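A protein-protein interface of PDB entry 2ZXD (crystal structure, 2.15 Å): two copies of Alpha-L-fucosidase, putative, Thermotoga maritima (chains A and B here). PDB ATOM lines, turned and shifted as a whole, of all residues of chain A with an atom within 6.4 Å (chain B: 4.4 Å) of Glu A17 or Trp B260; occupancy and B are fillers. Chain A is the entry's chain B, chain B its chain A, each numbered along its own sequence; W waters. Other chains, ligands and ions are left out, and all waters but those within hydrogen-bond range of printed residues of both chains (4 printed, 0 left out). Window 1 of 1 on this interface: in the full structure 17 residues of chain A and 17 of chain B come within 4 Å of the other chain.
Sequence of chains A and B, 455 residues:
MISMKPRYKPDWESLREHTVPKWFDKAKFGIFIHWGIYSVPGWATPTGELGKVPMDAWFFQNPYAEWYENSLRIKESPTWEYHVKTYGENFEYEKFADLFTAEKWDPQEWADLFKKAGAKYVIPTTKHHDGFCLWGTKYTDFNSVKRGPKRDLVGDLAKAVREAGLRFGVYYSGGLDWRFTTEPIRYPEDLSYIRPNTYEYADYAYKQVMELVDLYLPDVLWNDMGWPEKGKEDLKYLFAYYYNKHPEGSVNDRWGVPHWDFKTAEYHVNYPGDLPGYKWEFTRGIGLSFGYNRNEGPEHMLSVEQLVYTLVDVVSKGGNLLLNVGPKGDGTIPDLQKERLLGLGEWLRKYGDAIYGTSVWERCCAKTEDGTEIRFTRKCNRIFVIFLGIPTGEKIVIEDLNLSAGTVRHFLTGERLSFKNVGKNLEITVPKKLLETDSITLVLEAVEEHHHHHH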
ATOM      1  N   ARG A   7      37.993  26.915  12.840  1.00  0.00           N
ATOM      2  CA  ARG A   7      37.580  26.958  14.268  1.00  0.00           C
ATOM      3  C   ARG A   7      36.079  26.690  14.437  1.00  0.00           C
ATOM      4  O   ARG A   7      35.220  27.391  13.868  1.00  0.00           O
ATOM      5  CB  ARG A   7      37.894  28.325  14.880  1.00  0.00           C
ATOM      6  CG  ARG A   7      39.353  28.536  15.189  1.00  0.00           C
ATOM      7  CD  ARG A   7      39.960  27.407  16.011  1.00  0.00           C
ATOM      8  NE  ARG A   7      40.472  27.882  17.301  1.00  0.00           N
ATOM      9  CZ  ARG A   7      41.470  27.306  17.970  1.00  0.00           C
ATOM     10  NH1 ARG A   7      42.106  26.241  17.483  1.00  0.00           N
ATOM     11  NH2 ARG A   7      41.803  27.753  19.165  1.00  0.00           N
ATOM     12  N   TYR A   8      35.764  25.701  15.247  1.00  0.00           N
ATOM     13  CA  TYR A   8      34.370  25.388  15.503  1.00  0.00           C
ATOM     14  C   TYR A   8      33.941  26.214  16.705  1.00  0.00           C
ATOM     15  O   TYR A   8      34.750  26.503  17.598  1.00  0.00           O
ATOM     16  CB  TYR A   8      34.219  23.887  15.769  1.00  0.00           C
ATOM     17  CG  TYR A   8      34.557  23.076  14.535  1.00  0.00           C
ATOM     18  CD1 TYR A   8      33.620  22.921  13.504  1.00  0.00           C
ATOM     19  CD2 TYR A   8      35.825  22.497  14.379  1.00  0.00           C
ATOM     20  CE1 TYR A   8      33.940  22.210  12.354  1.00  0.00           C
ATOM     21  CE2 TYR A   8      36.153  21.780  13.223  1.00  0.00           C
ATOM     22  CZ  TYR A   8      35.203  21.643  12.216  1.00  0.00           C
ATOM     23  OH  TYR A   8      35.527  20.940  11.053  1.00  0.00           O
ATOM     24  N   TRP A  12      25.289  24.102  18.203  1.00  0.00           N
ATOM     25  CA  TRP A  12      24.949  23.035  17.274  1.00  0.00           C
ATOM     26  C   TRP A  12      25.048  23.388  15.780  1.00  0.00           C
ATOM     27  O   TRP A  12      25.534  22.589  14.985  1.00  0.00           O
ATOM     28  CB  TRP A  12      23.555  22.456  17.623  1.00  0.00           C
ATOM     29  CG  TRP A  12      23.366  22.059  19.096  1.00  0.00           C
ATOM     30  CD1 TRP A  12      22.380  22.507  19.931  1.00  0.00           C
ATOM     31  CD2 TRP A  12      24.211  21.179  19.902  1.00  0.00           C
ATOM     32  NE1 TRP A  12      22.566  21.988  21.195  1.00  0.00           N
ATOM     33  CE2 TRP A  12      23.669  21.172  21.214  1.00  0.00           C
ATOM     34  CE3 TRP A  12      25.350  20.410  19.634  1.00  0.00           C
ATOM     35  CZ2 TRP A  12      24.236  20.416  22.283  1.00  0.00           C
ATOM     36  CZ3 TRP A  12      25.934  19.640  20.698  1.00  0.00           C
ATOM     37  CH2 TRP A  12      25.363  19.660  22.013  1.00  0.00           C
ATOM     38  N   GLU A  13      24.658  24.600  15.417  1.00  0.00           N
ATOM     39  CA  GLU A  13      24.652  25.013  14.014  1.00  0.00           C
ATOM     40  C   GLU A  13      26.064  25.074  13.448  1.00  0.00           C
ATOM     41  O   GLU A  13      26.311  24.708  12.289  1.00  0.00           O
ATOM     42  CB  GLU A  13      23.907  26.371  13.868  1.00  0.00           C
ATOM     43  CG  GLU A  13      23.692  26.817  12.405  1.00  0.00           C
ATOM     44  CD  GLU A  13      22.810  28.116  12.242  1.00  0.00           C
ATOM     45  OE1 GLU A  13      22.357  28.397  11.103  1.00  0.00           O
ATOM     46  OE2 GLU A  13      22.587  28.842  13.251  1.00  0.00           O
ATOM     47  N   SER A  14      26.999  25.518  14.251  1.00  0.00           N
ATOM     48  CA  SER A  14      28.399  25.585  13.832  1.00  0.00           C
ATOM     49  C   SER A  14      29.050  24.202  13.842  1.00  0.00           C
ATOM     50  O   SER A  14      29.858  23.868  12.971  1.00  0.00           O
ATOM     51  CB  SER A  14      29.165  26.503  14.784  1.00  0.00           C
ATOM     52  OG  SER A  14      30.564  26.246  14.717  1.00  0.00           O
ATOM     53  N   LEU A  15      28.700  23.378  14.833  1.00  0.00           N
ATOM     54  CA  LEU A  15      29.289  22.042  14.913  1.00  0.00           C
ATOM     55  C   LEU A  15      28.866  21.179  13.711  1.00  0.00           C
ATOM     56  O   LEU A  15      29.594  20.267  13.326  1.00  0.00           O
ATOM     57  CB  LEU A  15      28.904  21.387  16.241  1.00  0.00           C
ATOM     58  CG  LEU A  15      29.631  22.076  17.421  1.00  0.00           C
ATOM     59  CD1 LEU A  15      28.964  21.672  18.762  1.00  0.00           C
ATOM     60  CD2 LEU A  15      31.077  21.650  17.441  1.00  0.00           C
ATOM     61  N   ARG A  16      27.706  21.509  13.110  1.00  0.00           N
ATOM     62  CA  ARG A  16      27.188  20.822  11.921  1.00  0.00           C
ATOM     63  C   ARG A  16      28.218  20.922  10.788  1.00  0.00           C
ATOM     64  O   ARG A  16      28.253  20.083   9.931  1.00  0.00           O
ATOM     65  CB  ARG A  16      25.812  21.422  11.486  1.00  0.00           C
ATOM     66  CG  ARG A  16      25.126  20.736  10.199  1.00  0.00           C
ATOM     67  CD  ARG A  16      24.550  19.294  10.490  1.00  0.00           C
ATOM     68  NE  ARG A  16      23.756  18.642   9.418  1.00  0.00           N
ATOM     69  CZ  ARG A  16      23.823  18.970   8.129  1.00  0.00           C
ATOM     70  NH1 ARG A  16      24.655  19.950   7.766  1.00  0.00           N
ATOM     71  NH2 ARG A  16      23.058  18.340   7.203  1.00  0.00           N
ATOM     72  N   GLU A  17      29.063  21.951  10.774  1.00  0.00           N
ATOM     73  CA  GLU A  17      30.115  22.056   9.757  1.00  0.00           C
ATOM     74  C   GLU A  17      31.131  20.893   9.819  1.00  0.00           C
ATOM     75  O   GLU A  17      31.865  20.648   8.844  1.00  0.00           O
ATOM     76  CB  GLU A  17      30.902  23.374   9.908  1.00  0.00           C
ATOM     77  CG  GLU A  17      30.026  24.621   9.778  1.00  0.00           C
ATOM     78  CD  GLU A  17      30.758  25.921  10.137  1.00  0.00           C
ATOM     79  OE1 GLU A  17      30.087  26.966  10.271  1.00  0.00           O
ATOM     80  OE2 GLU A  17      31.995  25.895  10.309  1.00  0.00           O
ATOM     81  N   HIS A  18      31.194  20.181  10.943  1.00  0.00           N
ATOM     82  CA  HIS A  18      32.141  19.063  11.041  1.00  0.00           C
ATOM     83  C   HIS A  18      31.479  17.810  10.500  1.00  0.00           C
ATOM     84  O   HIS A  18      30.498  17.322  11.033  1.00  0.00           O
ATOM     85  CB  HIS A  18      32.556  18.840  12.496  1.00  0.00           C
ATOM     86  CG  HIS A  18      33.508  17.708  12.684  1.00  0.00           C
ATOM     87  ND1 HIS A  18      33.091  16.395  12.786  1.00  0.00           N
ATOM     88  CD2 HIS A  18      34.863  17.674  12.679  1.00  0.00           C
ATOM     89  CE1 HIS A  18      34.149  15.600  12.824  1.00  0.00           C
ATOM     90  NE2 HIS A  18      35.237  16.348  12.755  1.00  0.00           N
ATOM     91  N   THR A  19      31.975  17.284   9.409  1.00  0.00           N
ATOM     92  CA  THR A  19      31.370  16.069   8.905  1.00  0.00           C
ATOM     93  C   THR A  19      32.286  14.875   9.240  1.00  0.00           C
ATOM     94  O   THR A  19      33.415  15.043   9.682  1.00  0.00           O
ATOM     95  CB  THR A  19      31.146  16.214   7.394  1.00  0.00           C
ATOM     96  OG1 THR A  19      32.313  16.779   6.787  1.00  0.00           O
ATOM     97  CG2 THR A  19      30.018  17.223   7.155  1.00  0.00           C
ATOM     98  N   HIS A 259      24.034  16.883  17.500  1.00  0.00           N
ATOM     99  CA  HIS A 259      25.174  16.530  16.713  1.00  0.00           C
ATOM    100  C   HIS A 259      25.762  15.118  16.878  1.00  0.00           C
ATOM    101  O   HIS A 259      25.695  14.512  17.961  1.00  0.00           O
ATOM    102  CB  HIS A 259      26.247  17.562  16.992  1.00  0.00           C
ATOM    103  CG  HIS A 259      27.472  17.381  16.166  1.00  0.00           C
ATOM    104  ND1 HIS A 259      27.518  17.715  14.832  1.00  0.00           N
ATOM    105  CD2 HIS A 259      28.672  16.821  16.465  1.00  0.00           C
ATOM    106  CE1 HIS A 259      28.693  17.368  14.342  1.00  0.00           C
ATOM    107  NE2 HIS A 259      29.410  16.824  15.314  1.00  0.00           N
ATOM    108  N   VAL B 251      17.849  22.698   2.151  1.00  0.00           N
ATOM    109  CA  VAL B 251      17.598  23.963   2.811  1.00  0.00           C
ATOM    110  C   VAL B 251      18.919  24.669   3.029  1.00  0.00           C
ATOM    111  O   VAL B 251      19.951  23.982   3.264  1.00  0.00           O
ATOM    112  CB  VAL B 251      16.821  23.775   4.196  1.00  0.00           C
ATOM    113  CG1 VAL B 251      15.620  22.832   3.989  1.00  0.00           C
ATOM    114  CG2 VAL B 251      17.762  23.244   5.346  1.00  0.00           C
ATOM    115  N   ASN B 252      18.895  26.020   3.005  1.00  0.00           N
ATOM    116  CA  ASN B 252      20.117  26.743   3.228  1.00  0.00           C
ATOM    117  C   ASN B 252      20.409  26.920   4.734  1.00  0.00           C
ATOM    118  O   ASN B 252      19.806  26.214   5.582  1.00  0.00           O
ATOM    119  CB  ASN B 252      20.128  28.066   2.471  1.00  0.00           C
ATOM    120  CG  ASN B 252      19.225  29.100   3.102  1.00  0.00           C
ATOM    121  OD1 ASN B 252      18.371  28.756   3.939  1.00  0.00           O
ATOM    122  ND2 ASN B 252      19.409  30.374   2.723  1.00  0.00           N
ATOM    123  N   ASP B 253      21.308  27.849   5.068  1.00  0.00           N
ATOM    124  CA  ASP B 253      21.744  28.013   6.443  1.00  0.00           C
ATOM    125  C   ASP B 253      21.384  29.349   7.105  1.00  0.00           C
ATOM    126  O   ASP B 253      22.104  29.815   8.000  1.00  0.00           O
ATOM    127  CB  ASP B 253      23.264  27.861   6.509  1.00  0.00           C
ATOM    128  CG  ASP B 253      23.999  29.044   5.894  1.00  0.00           C
ATOM    129  OD1 ASP B 253      25.163  29.287   6.257  1.00  0.00           O
ATOM    130  OD2 ASP B 253      23.436  29.721   5.007  1.00  0.00           O
ATOM    131  N   PRO B 258      19.778  24.573  14.488  1.00  0.00           N
ATOM    132  CA  PRO B 258      20.854  23.591  14.275  1.00  0.00           C
ATOM    133  C   PRO B 258      21.033  22.955  12.886  1.00  0.00           C
ATOM    134  O   PRO B 258      22.170  22.679  12.510  1.00  0.00           O
ATOM    135  CB  PRO B 258      20.586  22.510  15.354  1.00  0.00           C
ATOM    136  CG  PRO B 258      19.911  23.280  16.435  1.00  0.00           C
ATOM    137  CD  PRO B 258      18.939  24.173  15.641  1.00  0.00           C
ATOM    138  N   HIS B 259      19.972  22.748  12.117  1.00  0.00           N
ATOM    139  CA  HIS B 259      20.089  22.113  10.809  1.00  0.00           C
ATOM    140  C   HIS B 259      20.188  23.001   9.556  1.00  0.00           C
ATOM    141  O   HIS B 259      19.590  24.089   9.474  1.00  0.00           O
ATOM    142  CB  HIS B 259      18.897  21.161  10.619  1.00  0.00           C
ATOM    143  CG  HIS B 259      18.983  20.327   9.375  1.00  0.00           C
ATOM    144  ND1 HIS B 259      19.867  19.279   9.246  1.00  0.00           N
ATOM    145  CD2 HIS B 259      18.296  20.394   8.204  1.00  0.00           C
ATOM    146  CE1 HIS B 259      19.726  18.728   8.052  1.00  0.00           C
ATOM    147  NE2 HIS B 259      18.779  19.388   7.397  1.00  0.00           N
ATOM    148  N   TRP B 260      20.929  22.508   8.558  1.00  0.00           N
ATOM    149  CA  TRP B 260      21.058  23.138   7.251  1.00  0.00           C
ATOM    150  C   TRP B 260      21.770  22.096   6.373  1.00  0.00           C
ATOM    151  O   TRP B 260      22.455  21.213   6.911  1.00  0.00           O
ATOM    152  CB  TRP B 260      21.856  24.464   7.321  1.00  0.00           C
ATOM    153  CG  TRP B 260      23.136  24.386   8.079  1.00  0.00           C
ATOM    154  CD1 TRP B 260      23.343  24.781   9.367  1.00  0.00           C
ATOM    155  CD2 TRP B 260      24.409  23.911   7.597  1.00  0.00           C
ATOM    156  NE1 TRP B 260      24.668  24.585   9.728  1.00  0.00           N
ATOM    157  CE2 TRP B 260      25.340  24.046   8.662  1.00  0.00           C
ATOM    158  CE3 TRP B 260      24.858  23.385   6.371  1.00  0.00           C
ATOM    159  CZ2 TRP B 260      26.690  23.664   8.539  1.00  0.00           C
ATOM    160  CZ3 TRP B 260      26.210  23.001   6.262  1.00  0.00           C
ATOM    161  CH2 TRP B 260      27.100  23.141   7.335  1.00  0.00           C
ATOM    162  N   ASP B 261      21.570  22.144   5.054  1.00  0.00           N
ATOM    163  CA  ASP B 261      22.228  21.208   4.146  1.00  0.00           C
ATOM    164  C   ASP B 261      23.441  21.868   3.498  1.00  0.00           C
ATOM    165  O   ASP B 261      24.401  21.186   3.154  1.00  0.00           O
ATOM    166  CB  ASP B 261      21.285  20.715   3.066  1.00  0.00           C
ATOM    167  CG  ASP B 261      20.092  19.920   3.639  1.00  0.00           C
ATOM    168  OD1 ASP B 261      18.918  20.257   3.263  1.00  0.00           O
ATOM    169  OD2 ASP B 261      20.336  18.965   4.456  1.00  0.00           O
ATOM    170  N   PHE B 262      23.392  23.174   3.269  1.00  0.00           N
ATOM    171  CA  PHE B 262      24.550  23.881   2.726  1.00  0.00           C
ATOM    172  C   PHE B 262      24.654  25.273   3.318  1.00  0.00           C
ATOM    173  O   PHE B 262      23.636  25.904   3.713  1.00  0.00           O
ATOM    174  CB  PHE B 262      24.517  23.938   1.195  1.00  0.00           C
ATOM    175  CG  PHE B 262      23.321  24.708   0.611  1.00  0.00           C
ATOM    176  CD1 PHE B 262      23.423  26.076   0.349  1.00  0.00           C
ATOM    177  CD2 PHE B 262      22.088  24.045   0.362  1.00  0.00           C
ATOM    178  CE1 PHE B 262      22.311  26.795  -0.163  1.00  0.00           C
ATOM    179  CE2 PHE B 262      20.957  24.757  -0.144  1.00  0.00           C
ATOM    180  CZ  PHE B 262      21.085  26.145  -0.408  1.00  0.00           C
ATOM    181  N   LYS B 263      25.894  25.750   3.405  1.00  0.00           N
ATOM    182  CA  LYS B 263      26.145  27.089   3.922  1.00  0.00           C
ATOM    183  C   LYS B 263      26.114  28.137   2.796  1.00  0.00           C
ATOM    184  O   LYS B 263      26.295  27.808   1.623  1.00  0.00           O
ATOM    185  CB  LYS B 263      27.499  27.125   4.646  1.00  0.00           C
ATOM    186  CG  LYS B 263      27.408  26.467   6.072  1.00  0.00           C
ATOM    187  CD  LYS B 263      28.505  26.987   7.053  1.00  0.00           C
ATOM    188  CE  LYS B 263      28.304  28.481   7.493  1.00  0.00           C
ATOM    189  NZ  LYS B 263      26.973  28.634   8.219  1.00  0.00           N
ATOM    190  N   TYR B 278      32.438  21.236   4.164  1.00  0.00           N
ATOM    191  CA  TYR B 278      31.012  21.097   3.964  1.00  0.00           C
ATOM    192  C   TYR B 278      30.638  21.773   2.667  1.00  0.00           C
ATOM    193  O   TYR B 278      31.395  22.541   2.137  1.00  0.00           O
ATOM    194  CB  TYR B 278      30.301  21.756   5.139  1.00  0.00           C
ATOM    195  CG  TYR B 278      30.848  23.144   5.395  1.00  0.00           C
ATOM    196  CD1 TYR B 278      30.423  24.205   4.641  1.00  0.00           C
ATOM    197  CD2 TYR B 278      31.843  23.369   6.348  1.00  0.00           C
ATOM    198  CE1 TYR B 278      30.961  25.463   4.815  1.00  0.00           C
ATOM    199  CE2 TYR B 278      32.398  24.646   6.521  1.00  0.00           C
ATOM    200  CZ  TYR B 278      31.948  25.659   5.761  1.00  0.00           C
ATOM    201  OH  TYR B 278      32.420  26.935   5.930  1.00  0.00           O
ATOM    202  N   LYS B 279      29.466  21.459   2.162  1.00  0.00           N
ATOM    203  CA  LYS B 279      28.997  22.048   0.947  1.00  0.00           C
ATOM    204  C   LYS B 279      28.547  23.471   1.290  1.00  0.00           C
ATOM    205  O   LYS B 279      27.914  23.722   2.342  1.00  0.00           O
ATOM    206  CB  LYS B 279      27.819  21.260   0.389  1.00  0.00           C
ATOM    207  CG  LYS B 279      27.304  21.889  -0.925  1.00  0.00           C
ATOM    208  CD  LYS B 279      28.407  21.716  -2.073  1.00  0.00           C
ATOM    209  CE  LYS B 279      28.000  22.348  -3.411  1.00  0.00           C
ATOM    210  NZ  LYS B 279      29.190  22.418  -4.377  1.00  0.00           N
HETATM  211  O   HOH W   1      27.333  26.952  10.630  1.00  0.00           O
HETATM  212  O   HOH W   2      20.212  27.591   9.672  1.00  0.00           O
HETATM  213  O   HOH W   3      24.484  29.279   9.710  1.00  0.00           O
HETATM  214  O   HOH W   4      21.550  30.905  10.403  1.00  0.00           O
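OD1 of Asp B261 sits at hydrogen-bond distance from N of Val B251, 2.9 Å away. O of Phe B262 lies within hydrogen-bond range of N of Asp B253 (3.3 Å). NZ of Lys B263 lies within salt-bridge range of OD1 of Asp B253 (2.7 Å). A ring nitrogen (NE2) of His B259 is in hydrogen-bond range of the side-chain carboxylate (OD2) of Asp B261, 3.4 Å away. N of Lys B263 sits at hydrogen-bond distance from O of Lys B279 (3.1 Å).
NE1 of Trp B260 lies within hydrogen-bond range of O of Glu A13, at 3.0 Å. The guanidinium group of Arg A16 sits at hydrogen-bond distance from the backbone carbonyl oxygen of Trp B260, at 2.7 Å. OD2 of Asp B261 is in salt-bridge range of NH2 of Arg A16 (3.9 Å). The side-chain carboxylate (OE1) of Glu A13 lies close to the backbone carbonyl oxygen (O) of Asp B253, 3.4 Å away.
1 position is printed for both chains.
Printed residues of chain B that touch a printed residue of chain A: Asp B253, Pro B258, His B259, Trp B260, Asp B261, Lys B263 and Tyr B278. Hydrophobic or aromatic side chains of chain B that line the printed part of chain A: Pro B258, His B259, Trp B260 and Tyr B278. Hydrophobic or aromatic side chains of chain A that line the printed part of chain B: Trp A12. Among the printed residues, Asp or Glu carboxylates within 4 Å of a Lys or Arg side-chain nitrogen of the other chain: Arg A16 with Asp B261 (3.9 Å).
Among the printed residues, merely in contact across the chains: Arg A16 with His B259 (3.5 Å), Glu A17 with Lys B263 (3.6 Å), Glu A17 with Tyr B278 (3.7 Å), Glu A17 with Trp B260 (3.7 Å), Glu A13 with Pro B258 (3.7 Å), Trp A12 with Pro B258 (3.7 Å) and Arg A16 with Pro B258 (3.99 Å).
Water W3 lies within hydrogen-bond range of OE1 of Glu A13 (2.7 Å), NZ of Lys B263 (3.0 Å) and O of Asp B253 (3.0 Å). Water W4 bridges O of Asp B253 (2.7 Å) and OE1 of Glu A13 (2.7 Å). Water W2 bridges OE1 of Glu A13 (2.7 Å) and O of Asp B253 (3.4 Å). Water W1 lies within hydrogen-bond range of OE1 of Glu A17 (2.8 Å), NZ of Lys B263 (3.0 Å) and O of Glu A13 (3.0 Å).
Printed residues of chain B within 4 Å of Glu A17: Trp B260, Lys B263 and Tyr B278. Trp B260 touches three residues of chain A. Printed residues of chain B within 4 Å of Arg A16: Pro B258, His B259, Trp B260 and Asp B261. Printed residues of chain A within 4 Å of His B259: Arg A16. Printed residues of chain B within 4 Å of Glu A13: Asp B253 (3.4 Å), Pro B258 (3.7 Å) and Trp B260 (3.0 Å). Of the printed residues of chain A, Pro B258 touches Trp A12, Glu A13 and Arg A16. Printed residues of chain A within 4 Å of Lys B263: Glu A17 (3.6 Å). The nearest printed residue of chain B that does not touch Glu A17 is Asp B253 (6.8 Å). The nearest residue of chain A that does not touch Trp B260 is Ser A14 (5.2 Å).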
